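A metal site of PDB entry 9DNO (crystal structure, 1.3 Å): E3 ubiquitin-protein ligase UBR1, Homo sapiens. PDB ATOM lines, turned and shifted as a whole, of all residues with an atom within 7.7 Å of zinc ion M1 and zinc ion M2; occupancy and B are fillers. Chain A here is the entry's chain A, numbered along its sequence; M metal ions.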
ATOM      1  N   GLN A   6      25.369  23.805 -22.048  1.00  0.00           N
ATOM      2  CA  GLN A   6      24.277  23.497 -21.145  1.00  0.00           C
ATOM      3  C   GLN A   6      23.630  24.781 -20.651  1.00  0.00           C
ATOM      4  O   GLN A   6      24.310  25.795 -20.454  1.00  0.00           O
ATOM      5  CB  GLN A   6      24.764  22.721 -19.918  1.00  0.00           C
ATOM      6  CG  GLN A   6      25.160  21.294 -20.208  1.00  0.00           C
ATOM      7  CD  GLN A   6      25.996  20.699 -19.103  1.00  0.00           C
ATOM      8  OE1 GLN A   6      26.912  21.332 -18.569  1.00  0.00           O
ATOM      9  NE2 GLN A   6      25.697  19.450 -18.759  1.00  0.00           N
ATOM     10  N   LEU A   7      22.313  24.728 -20.484  1.00  0.00           N
ATOM     11  CA  LEU A   7      21.562  25.757 -19.785  1.00  0.00           C
ATOM     12  C   LEU A   7      21.497  25.341 -18.321  1.00  0.00           C
ATOM     13  O   LEU A   7      21.028  24.244 -18.002  1.00  0.00           O
ATOM     14  CB  LEU A   7      20.130  25.814 -20.326  1.00  0.00           C
ATOM     15  CG  LEU A   7      19.852  26.572 -21.614  1.00  0.00           C
ATOM     16  CD1 LEU A   7      18.395  26.369 -22.005  1.00  0.00           C
ATOM     17  CD2 LEU A   7      20.133  28.050 -21.446  1.00  0.00           C
ATOM     18  N   CYS A   8      21.953  26.211 -17.407  1.00  0.00           N
ATOM     19  CA  CYS A   8      21.946  25.838 -16.000  1.00  0.00           C
ATOM     20  C   CYS A   8      20.528  25.549 -15.515  1.00  0.00           C
ATOM     21  O   CYS A   8      20.246  24.445 -15.023  1.00  0.00           O
ATOM     22  CB  CYS A   8      22.573  26.951 -15.154  1.00  0.00           C
ATOM     23  SG  CYS A   8      22.429  26.584 -13.378  1.00  0.00           S
ATOM     24  N   GLY A   9      19.631  26.522 -15.654  1.00  0.00           N
ATOM     25  CA  GLY A   9      18.226  26.358 -15.305  1.00  0.00           C
ATOM     26  C   GLY A   9      17.923  26.223 -13.828  1.00  0.00           C
ATOM     27  O   GLY A   9      16.755  25.977 -13.489  1.00  0.00           O
ATOM     28  N   ARG A  10      18.908  26.382 -12.940  1.00  0.00           N
ATOM     29  CA  ARG A  10      18.654  26.249 -11.505  1.00  0.00           C
ATOM     30  C   ARG A  10      17.513  27.161 -11.067  1.00  0.00           C
ATOM     31  O   ARG A  10      17.563  28.368 -11.275  1.00  0.00           O
ATOM     32  CB  ARG A  10      19.911  26.606 -10.705  1.00  0.00           C
ATOM     33  CG  ARG A  10      19.608  26.951  -9.239  1.00  0.00           C
ATOM     34  CD  ARG A  10      20.311  26.043  -8.279  1.00  0.00           C
ATOM     35  NE  ARG A  10      19.864  26.259  -6.904  1.00  0.00           N
ATOM     36  CZ  ARG A  10      19.436  25.305  -6.096  1.00  0.00           C
ATOM     37  NH1 ARG A  10      19.430  24.028  -6.482  1.00  0.00           N
ATOM     38  NH2 ARG A  10      19.023  25.613  -4.872  1.00  0.00           N
ATOM     39  N   VAL A  11      16.497  26.582 -10.441  1.00  0.00           N
ATOM     40  CA  VAL A  11      15.401  27.353  -9.881  1.00  0.00           C
ATOM     41  C   VAL A  11      15.761  27.712  -8.440  1.00  0.00           C
ATOM     42  O   VAL A  11      16.108  26.833  -7.643  1.00  0.00           O
ATOM     43  CB  VAL A  11      14.092  26.552  -9.926  1.00  0.00           C
ATOM     44  CG1 VAL A  11      12.963  27.318  -9.234  1.00  0.00           C
ATOM     45  CG2 VAL A  11      13.725  26.206 -11.365  1.00  0.00           C
ATOM     46  N   PHE A  12      15.703  28.991  -8.101  1.00  0.00           N
ATOM     47  CA  PHE A  12      16.168  29.430  -6.796  1.00  0.00           C
ATOM     48  C   PHE A  12      15.148  29.114  -5.715  1.00  0.00           C
ATOM     49  O   PHE A  12      13.939  29.220  -5.927  1.00  0.00           O
ATOM     50  CB  PHE A  12      16.423  30.932  -6.785  1.00  0.00           C
ATOM     51  CG  PHE A  12      17.397  31.381  -7.827  1.00  0.00           C
ATOM     52  CD1 PHE A  12      18.686  30.883  -7.838  1.00  0.00           C
ATOM     53  CD2 PHE A  12      17.017  32.297  -8.790  1.00  0.00           C
ATOM     54  CE1 PHE A  12      19.591  31.293  -8.832  1.00  0.00           C
ATOM     55  CE2 PHE A  12      17.906  32.719  -9.762  1.00  0.00           C
ATOM     56  CZ  PHE A  12      19.190  32.202  -9.775  1.00  0.00           C
ATOM     57  N   VAL A  31      20.217  36.931 -14.161  1.00  0.00           N
ATOM     58  CA  VAL A  31      20.966  36.578 -12.963  1.00  0.00           C
ATOM     59  C   VAL A  31      21.651  35.241 -13.163  1.00  0.00           C
ATOM     60  O   VAL A  31      21.404  34.507 -14.119  1.00  0.00           O
ATOM     61  CB  VAL A  31      20.095  36.543 -11.683  1.00  0.00           C
ATOM     62  CG1 VAL A  31      19.779  37.948 -11.197  1.00  0.00           C
ATOM     63  CG2 VAL A  31      18.847  35.748 -11.931  1.00  0.00           C
ATOM     64  N   LEU A  32      22.489  34.931 -12.195  1.00  0.00           N
ATOM     65  CA  LEU A  32      23.262  33.696 -12.114  1.00  0.00           C
ATOM     66  C   LEU A  32      23.164  33.128 -10.697  1.00  0.00           C
ATOM     67  O   LEU A  32      23.116  33.875  -9.717  1.00  0.00           O
ATOM     68  CB  LEU A  32      24.769  33.946 -12.365  1.00  0.00           C
ATOM     69  CG  LEU A  32      25.083  34.465 -13.766  1.00  0.00           C
ATOM     70  CD1 LEU A  32      26.555  34.894 -13.853  1.00  0.00           C
ATOM     71  CD2 LEU A  32      24.802  33.386 -14.813  1.00  0.00           C
ATOM     72  N   CYS A  33      23.067  31.811 -10.611  1.00  0.00           N
ATOM     73  CA  CYS A  33      23.252  31.131  -9.330  1.00  0.00           C
ATOM     74  C   CYS A  33      24.691  31.274  -8.825  1.00  0.00           C
ATOM     75  O   CYS A  33      25.605  31.683  -9.548  1.00  0.00           O
ATOM     76  CB  CYS A  33      22.862  29.654  -9.433  1.00  0.00           C
ATOM     77  SG  CYS A  33      23.990  28.639 -10.408  1.00  0.00           S
ATOM     78  N   MET A  34      24.881  30.937  -7.553  1.00  0.00           N
ATOM     79  CA  MET A  34      26.189  31.146  -6.954  1.00  0.00           C
ATOM     80  C   MET A  34      27.276  30.340  -7.660  1.00  0.00           C
ATOM     81  O   MET A  34      28.359  30.869  -7.900  1.00  0.00           O
ATOM     82  CB  MET A  34      26.174  30.838  -5.459  1.00  0.00           C
ATOM     83  CG  MET A  34      27.531  31.100  -4.795  1.00  0.00           C
ATOM     84  SD  MET A  34      27.361  30.877  -3.031  1.00  0.00           S
ATOM     85  CE  MET A  34      26.085  32.071  -2.755  1.00  0.00           C
ATOM     86  N   ASP A  35      27.000  29.089  -8.002  1.00  0.00           N
ATOM     87  CA  ASP A  35      28.029  28.283  -8.655  1.00  0.00           C
ATOM     88  C   ASP A  35      28.379  28.851 -10.022  1.00  0.00           C
ATOM     89  O   ASP A  35      29.568  28.978 -10.366  1.00  0.00           O
ATOM     90  CB  ASP A  35      27.584  26.830  -8.754  1.00  0.00           C
ATOM     91  CG  ASP A  35      27.736  26.062  -7.452  1.00  0.00           C
ATOM     92  OD1 ASP A  35      28.403  26.585  -6.537  1.00  0.00           O
ATOM     93  OD2 ASP A  35      27.196  24.945  -7.344  1.00  0.00           O
ATOM     94  N   CYS A  36      27.383  29.255 -10.800  1.00  0.00           N
ATOM     95  CA  CYS A  36      27.706  29.784 -12.120  1.00  0.00           C
ATOM     96  C   CYS A  36      28.441  31.117 -12.017  1.00  0.00           C
ATOM     97  O   CYS A  36      29.397  31.370 -12.750  1.00  0.00           O
ATOM     98  CB  CYS A  36      26.449  29.921 -12.961  1.00  0.00           C
ATOM     99  SG  CYS A  36      25.693  28.343 -13.344  1.00  0.00           S
ATOM    100  N   PHE A  37      28.004  31.973 -11.089  1.00  0.00           N
ATOM    101  CA  PHE A  37      28.689  33.248 -10.901  1.00  0.00           C
ATOM    102  C   PHE A  37      30.151  33.035 -10.531  1.00  0.00           C
ATOM    103  O   PHE A  37      31.048  33.596 -11.174  1.00  0.00           O
ATOM    104  CB  PHE A  37      27.979  34.044  -9.798  1.00  0.00           C
ATOM    105  CG  PHE A  37      28.749  35.257  -9.359  1.00  0.00           C
ATOM    106  CD1 PHE A  37      28.854  36.359 -10.157  1.00  0.00           C
ATOM    107  CD2 PHE A  37      29.380  35.274  -8.122  1.00  0.00           C
ATOM    108  CE1 PHE A  37      29.578  37.482  -9.736  1.00  0.00           C
ATOM    109  CE2 PHE A  37      30.109  36.377  -7.714  1.00  0.00           C
ATOM    110  CZ  PHE A  37      30.191  37.474  -8.512  1.00  0.00           C
ATOM    111  N   ASP A  39      32.003  30.568 -11.035  1.00  0.00           N
ATOM    112  CA  ASP A  39      32.706  29.851 -12.088  1.00  0.00           C
ATOM    113  C   ASP A  39      32.698  30.583 -13.410  1.00  0.00           C
ATOM    114  O   ASP A  39      32.921  29.974 -14.461  1.00  0.00           O
ATOM    115  CB  ASP A  39      32.122  28.444 -12.256  1.00  0.00           C
ATOM    116  CG  ASP A  39      32.288  27.585 -11.016  1.00  0.00           C
ATOM    117  OD1 ASP A  39      33.100  27.957 -10.126  1.00  0.00           O
ATOM    118  OD2 ASP A  39      31.587  26.561 -10.890  1.00  0.00           O
ATOM    119  N   SER A  40      32.449  31.897 -13.392  1.00  0.00           N
ATOM    120  CA  SER A  40      32.278  32.690 -14.599  1.00  0.00           C
ATOM    121  C   SER A  40      33.177  33.915 -14.577  1.00  0.00           C
ATOM    122  O   SER A  40      33.740  34.286 -13.546  1.00  0.00           O
ATOM    123  CB  SER A  40      30.814  33.163 -14.776  1.00  0.00           C
ATOM    124  OG  SER A  40      30.507  34.207 -13.881  1.00  0.00           O
ATOM    125  N   PHE A  57      15.053  31.769 -12.063  1.00  0.00           N
ATOM    126  CA  PHE A  57      16.029  30.738 -12.348  1.00  0.00           C
ATOM    127  C   PHE A  57      17.285  31.380 -12.894  1.00  0.00           C
ATOM    128  O   PHE A  57      17.279  32.526 -13.360  1.00  0.00           O
ATOM    129  CB  PHE A  57      15.517  29.777 -13.432  1.00  0.00           C
ATOM    130  CG  PHE A  57      14.928  30.474 -14.635  1.00  0.00           C
ATOM    131  CD1 PHE A  57      13.738  31.207 -14.539  1.00  0.00           C
ATOM    132  CD2 PHE A  57      15.593  30.451 -15.843  1.00  0.00           C
ATOM    133  CE1 PHE A  57      13.206  31.856 -15.638  1.00  0.00           C
ATOM    134  CE2 PHE A  57      15.068  31.089 -16.955  1.00  0.00           C
ATOM    135  CZ  PHE A  57      13.872  31.803 -16.851  1.00  0.00           C
ATOM    136  N   CYS A  58      18.363  30.606 -12.829  1.00  0.00           N
ATOM    137  CA  CYS A  58      19.644  31.021 -13.364  1.00  0.00           C
ATOM    138  C   CYS A  58      19.617  31.134 -14.881  1.00  0.00           C
ATOM    139  O   CYS A  58      19.100  30.246 -15.574  1.00  0.00           O
ATOM    140  CB  CYS A  58      20.692  29.997 -12.945  1.00  0.00           C
ATOM    141  SG  CYS A  58      22.377  30.382 -13.519  1.00  0.00           S
ATOM    142  N   ASP A  59      20.191  32.214 -15.398  1.00  0.00           N
ATOM    143  CA  ASP A  59      20.256  32.461 -16.842  1.00  0.00           C
ATOM    144  C   ASP A  59      21.591  32.027 -17.452  1.00  0.00           C
ATOM    145  O   ASP A  59      21.861  32.384 -18.599  1.00  0.00           O
ATOM    146  CB  ASP A  59      20.025  33.931 -17.149  1.00  0.00           C
ATOM    147  CG  ASP A  59      18.650  34.414 -16.693  1.00  0.00           C
ATOM    148  OD1 ASP A  59      17.651  33.806 -17.161  1.00  0.00           O
ATOM    149  OD2 ASP A  59      18.573  35.376 -15.887  1.00  0.00           O
ATOM    150  N   CYS A  60      22.415  31.290 -16.727  1.00  0.00           N
ATOM    151  CA  CYS A  60      23.646  30.808 -17.319  1.00  0.00           C
ATOM    152  C   CYS A  60      23.343  29.930 -18.522  1.00  0.00           C
ATOM    153  O   CYS A  60      22.495  29.035 -18.456  1.00  0.00           O
ATOM    154  CB  CYS A  60      24.439  29.996 -16.309  1.00  0.00           C
ATOM    155  SG  CYS A  60      26.069  29.549 -16.953  1.00  0.00           S
ATOM    156  N   GLY A  61      24.038  30.201 -19.636  1.00  0.00           N
ATOM    157  CA  GLY A  61      23.872  29.454 -20.859  1.00  0.00           C
ATOM    158  C   GLY A  61      22.820  30.005 -21.789  1.00  0.00           C
ATOM    159  O   GLY A  61      22.639  29.490 -22.903  1.00  0.00           O
ATOM    160  N   PRO A  70      28.455  34.310 -21.701  1.00  0.00           N
ATOM    161  CA  PRO A  70      27.145  33.668 -21.485  1.00  0.00           C
ATOM    162  C   PRO A  70      27.206  32.342 -20.751  1.00  0.00           C
ATOM    163  O   PRO A  70      26.177  31.902 -20.220  1.00  0.00           O
ATOM    164  CB  PRO A  70      26.609  33.469 -22.910  1.00  0.00           C
ATOM    165  CG  PRO A  70      27.840  33.409 -23.732  1.00  0.00           C
ATOM    166  CD  PRO A  70      28.765  34.417 -23.132  1.00  0.00           C
ATOM    167  N   PHE A  71      28.351  31.678 -20.716  1.00  0.00           N
ATOM    168  CA  PHE A  71      28.483  30.402 -20.039  1.00  0.00           C
ATOM    169  C   PHE A  71      29.559  30.465 -18.966  1.00  0.00           C
ATOM    170  O   PHE A  71      30.642  30.994 -19.206  1.00  0.00           O
ATOM    171  CB  PHE A  71      28.938  29.307 -21.017  1.00  0.00           C
ATOM    172  CG  PHE A  71      27.958  29.024 -22.112  1.00  0.00           C
ATOM    173  CD1 PHE A  71      26.884  28.172 -21.890  1.00  0.00           C
ATOM    174  CD2 PHE A  71      28.133  29.563 -23.364  1.00  0.00           C
ATOM    175  CE1 PHE A  71      25.975  27.903 -22.915  1.00  0.00           C
ATOM    176  CE2 PHE A  71      27.244  29.290 -24.390  1.00  0.00           C
ATOM    177  CZ  PHE A  71      26.165  28.459 -24.156  1.00  0.00           C
ATOM    178  N   CYS A  72      29.278  29.901 -17.803  1.00  0.00           N
ATOM    179  CA  CYS A  72      30.327  29.608 -16.842  1.00  0.00           C
ATOM    180  C   CYS A  72      31.156  28.436 -17.370  1.00  0.00           C
ATOM    181  O   CYS A  72      30.787  27.756 -18.335  1.00  0.00           O
ATOM    182  CB  CYS A  72      29.740  29.319 -15.452  1.00  0.00           C
ATOM    183  SG  CYS A  72      28.996  27.736 -15.343  1.00  0.00           S
ATOM    184  N   VAL A  73      32.297  28.184 -16.720  1.00  0.00           N
ATOM    185  CA  VAL A  73      33.175  27.108 -17.198  1.00  0.00           C
ATOM    186  C   VAL A  73      32.526  25.725 -17.058  1.00  0.00           C
ATOM    187  O   VAL A  73      32.858  24.815 -17.817  1.00  0.00           O
ATOM    188  CB  VAL A  73      34.591  27.174 -16.601  1.00  0.00           C
ATOM    189  CG1 VAL A  73      35.301  28.465 -16.996  1.00  0.00           C
ATOM    190  CG2 VAL A  73      34.541  27.012 -15.116  1.00  0.00           C
ATOM    191  N   ASN A  74      31.585  25.549 -16.115  1.00  0.00           N
ATOM    192  CA  ASN A  74      30.887  24.267 -16.021  1.00  0.00           C
ATOM    193  C   ASN A  74      29.906  24.032 -17.170  1.00  0.00           C
ATOM    194  O   ASN A  74      29.692  22.873 -17.564  1.00  0.00           O
ATOM    195  CB  ASN A  74      30.186  24.107 -14.672  1.00  0.00           C
ATOM    196  CG  ASN A  74      31.049  23.370 -13.676  1.00  0.00           C
ATOM    197  OD1 ASN A  74      31.739  22.416 -14.051  1.00  0.00           O
ATOM    198  ND2 ASN A  74      30.998  23.787 -12.424  1.00  0.00           N
ATOM    199  N   HIS A  75      29.287  25.068 -17.705  1.00  0.00           N
ATOM    200  CA  HIS A  75      28.191  24.892 -18.641  1.00  0.00           C
ATOM    201  C   HIS A  75      28.602  25.191 -20.072  1.00  0.00           C
ATOM    202  O   HIS A  75      27.798  24.975 -20.984  1.00  0.00           O
ATOM    203  CB  HIS A  75      26.990  25.722 -18.170  1.00  0.00           C
ATOM    204  CG  HIS A  75      26.417  25.231 -16.866  1.00  0.00           C
ATOM    205  ND1 HIS A  75      26.104  26.050 -15.806  1.00  0.00           N
ATOM    206  CD2 HIS A  75      26.140  23.968 -16.454  1.00  0.00           C
ATOM    207  CE1 HIS A  75      25.633  25.316 -14.808  1.00  0.00           C
ATOM    208  NE2 HIS A  75      25.630  24.047 -15.184  1.00  0.00           N
ATOM    209  N   GLU A  76      29.828  25.668 -20.285  1.00  0.00           N
ATOM    210  CA  GLU A  76      30.275  25.998 -21.613  1.00  0.00           C
ATOM    211  C   GLU A  76      30.435  24.726 -22.450  1.00  0.00           C
ATOM    212  O   GLU A  76      30.595  23.635 -21.913  1.00  0.00           O
ATOM    213  CB  GLU A  76      31.625  26.712 -21.540  1.00  0.00           C
ATOM    214  CG  GLU A  76      32.701  25.896 -20.905  1.00  0.00           C
ATOM    215  CD  GLU A  76      34.049  26.517 -21.105  1.00  0.00           C
ATOM    216  OE1 GLU A  76      34.130  27.764 -21.007  1.00  0.00           O
ATOM    217  OE2 GLU A  76      35.030  25.770 -21.335  1.00  0.00           O
HETATM  218 ZN    ZN M   1      26.708  27.935 -15.480  1.00  0.00          ZN
HETATM  219 ZN    ZN M   2      23.438  28.483 -12.653  1.00  0.00          ZN
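The backbone carbonyl oxygen (O) of His 75 is in hydrogen-bond range of the backbone NH (N) of Gln 6 (2.9 Å).
N of Cys 8 is in hydrogen-bond range of O of Cys 60 (3.1 Å).
The backbone NH (N) of Arg 10 sits close to the side-chain sulfur (SG) of Cys 8, 3.6 Å away.
The side-chain sulfur (SG) of Cys 58 lies close to the backbone NH (N) of Cys 60, 3.3 Å away.
SG of Cys 72 lies close to N of Asn 74, 3.5 Å away.
The backbone NH (N) of Cys 58 is in hydrogen-bond range of the backbone carbonyl oxygen (O) of Arg 10 (2.8 Å).
The side-chain hydroxyl (OG) of Ser 40 sits close to the backbone carbonyl oxygen (O) of Cys 36, 3.2 Å away.
Zinc ion M2 is bound by SG of Cys 8 (2.3 Å), SG of Cys 33 (2.3 Å), SG of Cys 58 (2.3 Å) and SG of Cys 36 (2.4 Å).
Zinc ion M2 has four donor atoms within binding distance.
Zinc ion M1 is bound by ND1 of His 75 (2.0 Å), SG of Cys 60 (2.3 Å), SG of Cys 72 (2.3 Å) and SG of Cys 36 (2.4 Å).
Zinc ion M1 has four donor atoms within binding distance.
Of the 28 residues printed, 4 come within 4 Å of zinc ion M1.
The nearest printed residue that does not touch zinc ion M1 is Cys 8 (4.3 Å).
Of the 28 residues printed, 4 come within 4 Å of zinc ion M2.
The nearest printed residue that does not touch zinc ion M2 is Cys 60 (4.1 Å).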
